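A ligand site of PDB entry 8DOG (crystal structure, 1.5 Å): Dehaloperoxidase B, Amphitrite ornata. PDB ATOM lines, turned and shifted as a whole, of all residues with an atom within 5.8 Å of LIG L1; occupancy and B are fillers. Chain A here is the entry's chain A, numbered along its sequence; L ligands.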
ATOM      1  N   TYR A  16      20.024 -29.879  -6.015  1.00  0.00           N
ATOM      2  CA  TYR A  16      20.786 -30.845  -6.814  1.00  0.00           C
ATOM      3  C   TYR A  16      21.808 -30.129  -7.706  1.00  0.00           C
ATOM      4  O   TYR A  16      22.933 -30.621  -7.938  1.00  0.00           O
ATOM      5  CB  TYR A  16      19.845 -31.685  -7.679  1.00  0.00           C
ATOM      6  CG  TYR A  16      19.062 -32.726  -6.950  1.00  0.00           C
ATOM      7  CD1 TYR A  16      19.728 -33.786  -6.358  1.00  0.00           C
ATOM      8  CD2 TYR A  16      17.683 -32.714  -6.904  1.00  0.00           C
ATOM      9  CE1 TYR A  16      19.039 -34.808  -5.741  1.00  0.00           C
ATOM     10  CE2 TYR A  16      16.983 -33.723  -6.262  1.00  0.00           C
ATOM     11  CZ  TYR A  16      17.669 -34.771  -5.652  1.00  0.00           C
ATOM     12  OH  TYR A  16      17.015 -35.815  -5.037  1.00  0.00           O
ATOM     13  N   ALA A  17      21.423 -28.960  -8.242  1.00  0.00           N
ATOM     14  CA  ALA A  17      22.323 -28.219  -9.173  1.00  0.00           C
ATOM     15  C   ALA A  17      23.620 -27.864  -8.452  1.00  0.00           C
ATOM     16  O   ALA A  17      24.716 -28.100  -8.958  1.00  0.00           O
ATOM     17  CB  ALA A  17      21.670 -26.911  -9.624  1.00  0.00           C
ATOM     18  N   GLN A  18      23.471 -27.373  -7.221  1.00  0.00           N
ATOM     19  CA  GLN A  18      24.665 -26.966  -6.425  1.00  0.00           C
ATOM     20  C   GLN A  18      25.456 -28.185  -5.972  1.00  0.00           C
ATOM     21  O   GLN A  18      26.673 -28.207  -6.117  1.00  0.00           O
ATOM     22  CB  GLN A  18      24.246 -26.144  -5.221  1.00  0.00           C
ATOM     23  CG  GLN A  18      23.704 -24.771  -5.624  1.00  0.00           C
ATOM     24  CD  GLN A  18      23.318 -23.951  -4.418  1.00  0.00           C
ATOM     25  OE1 GLN A  18      23.264 -24.400  -3.273  1.00  0.00           O
ATOM     26  NE2 GLN A  18      22.995 -22.726  -4.616  1.00  0.00           N
ATOM     27  N   ILE A  20      25.611 -31.297  -7.163  1.00  0.00           N
ATOM     28  CA  ILE A  20      26.320 -32.040  -8.245  1.00  0.00           C
ATOM     29  C   ILE A  20      27.500 -31.221  -8.750  1.00  0.00           C
ATOM     30  O   ILE A  20      28.525 -31.812  -9.028  1.00  0.00           O
ATOM     31  CB  ILE A  20      25.303 -32.397  -9.355  1.00  0.00           C
ATOM     32  CG1 ILE A  20      24.337 -33.453  -8.825  1.00  0.00           C
ATOM     33  CG2 ILE A  20      26.009 -32.847 -10.627  1.00  0.00           C
ATOM     34  CD1 ILE A  20      23.090 -33.685  -9.704  1.00  0.00           C
ATOM     35  N   PHE A  21      27.349 -29.891  -8.888  1.00  0.00           N
ATOM     36  CA  PHE A  21      28.500 -29.101  -9.309  1.00  0.00           C
ATOM     37  C   PHE A  21      29.634 -29.182  -8.278  1.00  0.00           C
ATOM     38  O   PHE A  21      30.810 -29.298  -8.648  1.00  0.00           O
ATOM     39  CB  PHE A  21      28.095 -27.664  -9.536  1.00  0.00           C
ATOM     40  CG  PHE A  21      29.221 -26.792 -10.062  1.00  0.00           C
ATOM     41  CD1 PHE A  21      30.079 -27.179 -11.067  1.00  0.00           C
ATOM     42  CD2 PHE A  21      29.465 -25.578  -9.459  1.00  0.00           C
ATOM     43  CE1 PHE A  21      31.098 -26.361 -11.525  1.00  0.00           C
ATOM     44  CE2 PHE A  21      30.449 -24.726  -9.923  1.00  0.00           C
ATOM     45  CZ  PHE A  21      31.293 -25.118 -10.937  1.00  0.00           C
ATOM     46  N   PHE A  24      31.430 -32.395  -8.665  1.00  0.00           N
ATOM     47  CA  PHE A  24      32.365 -32.266  -9.801  1.00  0.00           C
ATOM     48  C   PHE A  24      33.622 -31.496  -9.417  1.00  0.00           C
ATOM     49  O   PHE A  24      34.720 -31.993  -9.738  1.00  0.00           O
ATOM     50  CB  PHE A  24      31.566 -31.635 -10.933  1.00  0.00           C
ATOM     51  CG  PHE A  24      32.405 -31.173 -12.095  1.00  0.00           C
ATOM     52  CD1 PHE A  24      33.069 -32.060 -12.909  1.00  0.00           C
ATOM     53  CD2 PHE A  24      32.512 -29.814 -12.393  1.00  0.00           C
ATOM     54  CE1 PHE A  24      33.797 -31.628 -14.008  1.00  0.00           C
ATOM     55  CE2 PHE A  24      33.214 -29.382 -13.506  1.00  0.00           C
ATOM     56  CZ  PHE A  24      33.876 -30.280 -14.312  1.00  0.00           C
ATOM     57  N   PHE A  35      36.720 -21.695 -13.612  1.00  0.00           N
ATOM     58  CA  PHE A  35      35.822 -21.036 -12.635  1.00  0.00           C
ATOM     59  C   PHE A  35      36.641 -20.308 -11.572  1.00  0.00           C
ATOM     60  O   PHE A  35      36.581 -20.649 -10.417  1.00  0.00           O
ATOM     61  CB  PHE A  35      34.932 -22.069 -11.942  1.00  0.00           C
ATOM     62  CG  PHE A  35      34.163 -22.921 -12.881  1.00  0.00           C
ATOM     63  CD1 PHE A  35      33.050 -22.404 -13.500  1.00  0.00           C
ATOM     64  CD2 PHE A  35      34.579 -24.210 -13.194  1.00  0.00           C
ATOM     65  CE1 PHE A  35      32.331 -23.206 -14.360  1.00  0.00           C
ATOM     66  CE2 PHE A  35      33.880 -24.973 -14.104  1.00  0.00           C
ATOM     67  CZ  PHE A  35      32.748 -24.464 -14.668  1.00  0.00           C
ATOM     68  N   TYR A  38      35.647 -19.136  -8.082  1.00  0.00           N
ATOM     69  CA  TYR A  38      35.269 -20.183  -7.075  1.00  0.00           C
ATOM     70  C   TYR A  38      36.461 -20.750  -6.315  1.00  0.00           C
ATOM     71  O   TYR A  38      36.268 -21.609  -5.414  1.00  0.00           O
ATOM     72  CB  TYR A  38      34.423 -21.279  -7.703  1.00  0.00           C
ATOM     73  CG  TYR A  38      33.181 -20.796  -8.392  1.00  0.00           C
ATOM     74  CD1 TYR A  38      32.550 -19.625  -8.048  1.00  0.00           C
ATOM     75  CD2 TYR A  38      32.607 -21.562  -9.394  1.00  0.00           C
ATOM     76  CE1 TYR A  38      31.379 -19.215  -8.671  1.00  0.00           C
ATOM     77  CE2 TYR A  38      31.460 -21.147 -10.053  1.00  0.00           C
ATOM     78  CZ  TYR A  38      30.831 -19.978  -9.700  1.00  0.00           C
ATOM     79  OH  TYR A  38      29.720 -19.541 -10.375  1.00  0.00           O
ATOM     80  N   LYS A  51      26.523 -15.557  -7.749  1.00  0.00           N
ATOM     81  CA  LYS A  51      26.617 -16.091  -9.119  1.00  0.00           C
ATOM     82  C   LYS A  51      26.740 -17.607  -9.058  1.00  0.00           C
ATOM     83  O   LYS A  51      26.338 -18.281  -9.981  1.00  0.00           O
ATOM     84  CB  LYS A  51      27.783 -15.479  -9.886  1.00  0.00           C
ATOM     85  CG  LYS A  51      27.559 -14.017 -10.161  1.00  0.00           C
ATOM     86  CD  LYS A  51      28.624 -13.407 -10.977  1.00  0.00           C
ATOM     87  CE  LYS A  51      28.351 -11.938 -11.125  1.00  0.00           C
ATOM     88  NZ  LYS A  51      29.305 -11.311 -12.078  1.00  0.00           N
ATOM     89  N   PHE A  52      27.315 -18.152  -8.004  1.00  0.00           N
ATOM     90  CA  PHE A  52      27.369 -19.623  -7.929  1.00  0.00           C
ATOM     91  C   PHE A  52      25.955 -20.175  -7.855  1.00  0.00           C
ATOM     92  O   PHE A  52      25.642 -21.093  -8.652  1.00  0.00           O
ATOM     93  CB  PHE A  52      28.109 -19.990  -6.656  1.00  0.00           C
ATOM     94  CG  PHE A  52      28.179 -21.480  -6.432  1.00  0.00           C
ATOM     95  CD1 PHE A  52      29.257 -22.213  -6.891  1.00  0.00           C
ATOM     96  CD2 PHE A  52      27.183 -22.106  -5.698  1.00  0.00           C
ATOM     97  CE1 PHE A  52      29.319 -23.576  -6.613  1.00  0.00           C
ATOM     98  CE2 PHE A  52      27.240 -23.463  -5.479  1.00  0.00           C
ATOM     99  CZ  PHE A  52      28.301 -24.179  -5.943  1.00  0.00           C
ATOM    100  N   HIS A  55      24.127 -19.199 -11.456  1.00  0.00           N
ATOM    101  CA  HIS A  55      24.723 -19.861 -12.643  1.00  0.00           C
ATOM    102  C   HIS A  55      24.454 -21.361 -12.518  1.00  0.00           C
ATOM    103  O   HIS A  55      24.057 -21.968 -13.504  1.00  0.00           O
ATOM    104  CB  HIS A  55      26.188 -19.516 -12.869  1.00  0.00           C
ATOM    105  CG  HIS A  55      26.400 -18.096 -13.327  1.00  0.00           C
ATOM    106  ND1 HIS A  55      27.283 -17.779 -14.325  1.00  0.00           N
ATOM    107  CD2 HIS A  55      25.849 -16.926 -12.929  1.00  0.00           C
ATOM    108  CE1 HIS A  55      27.289 -16.478 -14.526  1.00  0.00           C
ATOM    109  NE2 HIS A  55      26.444 -15.925 -13.662  1.00  0.00           N
ATOM    110  N   THR A  56      24.715 -21.974 -11.381  1.00  0.00           N
ATOM    111  CA  THR A  56      24.466 -23.429 -11.242  1.00  0.00           C
ATOM    112  C   THR A  56      23.038 -23.737 -11.602  1.00  0.00           C
ATOM    113  O   THR A  56      22.796 -24.732 -12.294  1.00  0.00           O
ATOM    114  CB  THR A  56      24.878 -23.987  -9.871  1.00  0.00           C
ATOM    115  OG1 THR A  56      24.097 -23.396  -8.828  1.00  0.00           O
ATOM    116  CG2 THR A  56      26.373 -23.874  -9.736  1.00  0.00           C
ATOM    117  N   GLU A  57      22.102 -22.960 -11.117  1.00  0.00           N
ATOM    118  CA  GLU A  57      20.695 -23.252 -11.386  1.00  0.00           C
ATOM    119  C   GLU A  57      20.355 -23.039 -12.873  1.00  0.00           C
ATOM    120  O   GLU A  57      19.577 -23.860 -13.388  1.00  0.00           O
ATOM    121  CB  GLU A  57      19.776 -22.440 -10.503  1.00  0.00           C
ATOM    122  CG  GLU A  57      18.347 -22.790 -10.745  1.00  0.00           C
ATOM    123  CD  GLU A  57      17.429 -22.566  -9.575  1.00  0.00           C
ATOM    124  OE1 GLU A  57      16.311 -23.062  -9.634  1.00  0.00           O
ATOM    125  OE2 GLU A  57      17.844 -21.941  -8.621  1.00  0.00           O
ATOM    126  N   VAL A  59      22.431 -23.405 -15.422  1.00  0.00           N
ATOM    127  CA  VAL A  59      23.088 -24.535 -16.098  1.00  0.00           C
ATOM    128  C   VAL A  59      22.173 -25.745 -15.970  1.00  0.00           C
ATOM    129  O   VAL A  59      21.900 -26.438 -16.958  1.00  0.00           O
ATOM    130  CB  VAL A  59      24.493 -24.830 -15.552  1.00  0.00           C
ATOM    131  CG1 VAL A  59      25.003 -26.177 -16.074  1.00  0.00           C
ATOM    132  CG2 VAL A  59      25.454 -23.705 -15.872  1.00  0.00           C
ATOM    133  N   PHE A  60      21.750 -26.070 -14.769  1.00  0.00           N
ATOM    134  CA  PHE A  60      20.997 -27.302 -14.547  1.00  0.00           C
ATOM    135  C   PHE A  60      19.608 -27.230 -15.166  1.00  0.00           C
ATOM    136  O   PHE A  60      19.088 -28.253 -15.619  1.00  0.00           O
ATOM    137  CB  PHE A  60      20.937 -27.525 -13.040  1.00  0.00           C
ATOM    138  CG  PHE A  60      20.753 -28.931 -12.617  1.00  0.00           C
ATOM    139  CD1 PHE A  60      21.835 -29.817 -12.666  1.00  0.00           C
ATOM    140  CD2 PHE A  60      19.489 -29.367 -12.267  1.00  0.00           C
ATOM    141  CE1 PHE A  60      21.618 -31.140 -12.336  1.00  0.00           C
ATOM    142  CE2 PHE A  60      19.304 -30.694 -11.904  1.00  0.00           C
ATOM    143  CZ  PHE A  60      20.358 -31.567 -11.986  1.00  0.00           C
ATOM    144  N   MET A  63      20.348 -28.221 -18.607  1.00  0.00           N
ATOM    145  CA  MET A  63      20.757 -29.625 -18.667  1.00  0.00           C
ATOM    146  C   MET A  63      19.457 -30.478 -18.649  1.00  0.00           C
ATOM    147  O   MET A  63      19.402 -31.526 -19.352  1.00  0.00           O
ATOM    148  CB  MET A  63      21.692 -30.009 -17.494  1.00  0.00           C
ATOM    149  CG  MET A  63      22.246 -31.393 -17.637  1.00  0.00           C
ATOM    150  SD  MET A  63      23.005 -31.969 -16.101  1.00  0.00           S
ATOM    151  CE  MET A  63      24.353 -30.802 -15.891  1.00  0.00           C
ATOM    152  N   LEU A 100      32.218 -34.031 -15.879  1.00  0.00           N
ATOM    153  CA  LEU A 100      30.959 -33.664 -15.251  1.00  0.00           C
ATOM    154  C   LEU A 100      30.036 -34.871 -15.120  1.00  0.00           C
ATOM    155  O   LEU A 100      29.474 -35.053 -14.029  1.00  0.00           O
ATOM    156  CB  LEU A 100      30.317 -32.504 -15.988  1.00  0.00           C
ATOM    157  CG  LEU A 100      28.930 -32.089 -15.519  1.00  0.00           C
ATOM    158  CD1 LEU A 100      28.953 -31.677 -14.061  1.00  0.00           C
ATOM    159  CD2 LEU A 100      28.350 -31.003 -16.408  1.00  0.00           C
HETATM  160  C1  LIG L   1      29.679 -26.810 -15.044  1.00  0.00           C
HETATM  161  C2  LIG L   1      25.505 -27.137 -12.324  1.00  0.00           C
HETATM  162  C3  LIG L   1      26.892 -29.018 -12.684  1.00  0.00           C
HETATM  163  C4  LIG L   1      28.967 -22.291 -14.611  1.00  0.00           C
HETATM  164  C5  LIG L   1      28.732 -22.976 -12.318  1.00  0.00           C
HETATM  165  C6  LIG L   1      26.357 -26.379 -13.138  1.00  0.00           C
HETATM  166  C7  LIG L   1      27.768 -28.262 -13.451  1.00  0.00           C
HETATM  167  C8  LIG L   1      28.809 -23.603 -15.032  1.00  0.00           C
HETATM  168  C9  LIG L   1      28.620 -24.303 -12.752  1.00  0.00           C
HETATM  169  C10 LIG L   1      25.743 -28.480 -12.136  1.00  0.00           C
HETATM  170  C11 LIG L   1      28.981 -21.985 -13.252  1.00  0.00           C
HETATM  171  C12 LIG L   1      27.517 -26.909 -13.697  1.00  0.00           C
HETATM  172  C13 LIG L   1      28.637 -24.652 -14.105  1.00  0.00           C
HETATM  173  C14 LIG L   1      28.411 -26.073 -14.601  1.00  0.00           C
HETATM  174  O1  LIG L   1      24.876 -29.199 -11.344  1.00  0.00           O
HETATM  175  O2  LIG L   1      29.200 -20.703 -12.850  1.00  0.00           O
HETATM  176  C1  LG2 L   2      27.955 -21.063 -18.539  1.00  0.00           C
HETATM  177  C2  LG2 L   2      24.860 -24.714 -19.606  1.00  0.00           C
HETATM  178  C3  LG2 L   2      28.485 -27.907 -19.015  1.00  0.00           C
HETATM  179  C4  LG2 L   2      31.576 -24.236 -18.174  1.00  0.00           C
HETATM  180  C5  LG2 L   2      26.773 -21.794 -18.820  1.00  0.00           C
HETATM  181  C6  LG2 L   2      25.429 -21.251 -18.912  1.00  0.00           C
HETATM  182  C7  LG2 L   2      24.542 -22.317 -19.224  1.00  0.00           C
HETATM  183  C8  LG2 L   2      25.391 -23.435 -19.330  1.00  0.00           C
HETATM  184  C9  LG2 L   2      23.046 -22.179 -19.421  1.00  0.00           C
HETATM  185  C10 LG2 L   2      25.057 -19.805 -18.625  1.00  0.00           C
HETATM  186  C11 LG2 L   2      24.924 -19.576 -17.119  1.00  0.00           C
HETATM  187  C12 LG2 L   2      24.578 -18.172 -16.699  1.00  0.00           C
HETATM  188  O1  LG2 L   2      24.010 -17.893 -15.623  1.00  0.00           O
HETATM  189  O2  LG2 L   2      25.029 -17.209 -17.394  1.00  0.00           O
HETATM  190  C13 LG2 L   2      25.586 -25.877 -19.555  1.00  0.00           C
HETATM  191  C14 LG2 L   2      24.962 -27.206 -19.723  1.00  0.00           C
HETATM  192  C15 LG2 L   2      25.973 -28.079 -19.503  1.00  0.00           C
HETATM  193  C16 LG2 L   2      27.249 -27.356 -19.267  1.00  0.00           C
HETATM  194  C17 LG2 L   2      23.495 -27.515 -19.918  1.00  0.00           C
HETATM  195  C18 LG2 L   2      26.029 -29.556 -19.492  1.00  0.00           C
HETATM  196  C19 LG2 L   2      25.155 -30.283 -20.219  1.00  0.00           C
HETATM  197  C20 LG2 L   2      29.598 -27.155 -18.694  1.00  0.00           C
HETATM  198  C21 LG2 L   2      30.855 -27.733 -18.337  1.00  0.00           C
HETATM  199  C22 LG2 L   2      31.734 -26.690 -18.100  1.00  0.00           C
HETATM  200  C23 LG2 L   2      30.986 -25.497 -18.297  1.00  0.00           C
HETATM  201  C24 LG2 L   2      31.202 -29.236 -18.347  1.00  0.00           C
HETATM  202  C25 LG2 L   2      33.125 -26.754 -17.710  1.00  0.00           C
HETATM  203  C26 LG2 L   2      33.685 -27.792 -17.057  1.00  0.00           C
HETATM  204  C27 LG2 L   2      30.767 -23.091 -18.302  1.00  0.00           C
HETATM  205  C28 LG2 L   2      31.382 -21.765 -18.049  1.00  0.00           C
HETATM  206  C29 LG2 L   2      30.370 -20.882 -18.131  1.00  0.00           C
HETATM  207  C30 LG2 L   2      29.158 -21.650 -18.359  1.00  0.00           C
HETATM  208  C31 LG2 L   2      32.844 -21.515 -17.769  1.00  0.00           C
HETATM  209  C32 LG2 L   2      30.374 -19.361 -18.024  1.00  0.00           C
HETATM  210  C33 LG2 L   2      30.944 -18.839 -16.760  1.00  0.00           C
HETATM  211  C34 LG2 L   2      29.964 -19.065 -15.671  1.00  0.00           C
HETATM  212  O3  LG2 L   2      28.753 -19.151 -15.911  1.00  0.00           O
HETATM  213  O4  LG2 L   2      30.410 -19.154 -14.449  1.00  0.00           O
HETATM  214  N1  LG2 L   2      26.734 -23.163 -19.070  1.00  0.00           N
HETATM  215  N2  LG2 L   2      26.925 -26.026 -19.323  1.00  0.00           N
HETATM  216  N3  LG2 L   2      29.688 -25.819 -18.648  1.00  0.00           N
HETATM  217  N4  LG2 L   2      29.450 -22.958 -18.552  1.00  0.00           N
HETATM  218 FE1  LG2 L   2      28.240 -24.449 -19.161  1.00  0.00          FE
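The backbone carbonyl oxygen (O) of Ala 17 lies within hydrogen-bond range of an oxygen (O1) of LIG L1, at 2.6 Å.
The side-chain hydroxyl of Tyr 38 sits at hydrogen-bond distance from an oxygen (O2) of LIG L1, 2.8 Å away.
ND1 of His 55 is in hydrogen-bond range of O3 of LG2 L2.
Residues that only touch LIG L1: His 55 (3.2 Å), Val 59 (3.2 Å), Phe 21 (3.3 Å), Phe 60 (3.4 Å), Phe 35 (3.5 Å), Thr 56 (3.6 Å), Leu 100 (3.6 Å) and Ile 20 (3.8 Å).
O2 of LIG L1 is in hydrogen-bond range of O4 of LG2 L2, at 2.5 Å.
The side-chain hydroxyl of Thr 56 lies within hydrogen-bond range of the backbone carbonyl oxygen of Phe 52, at 2.8 Å.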
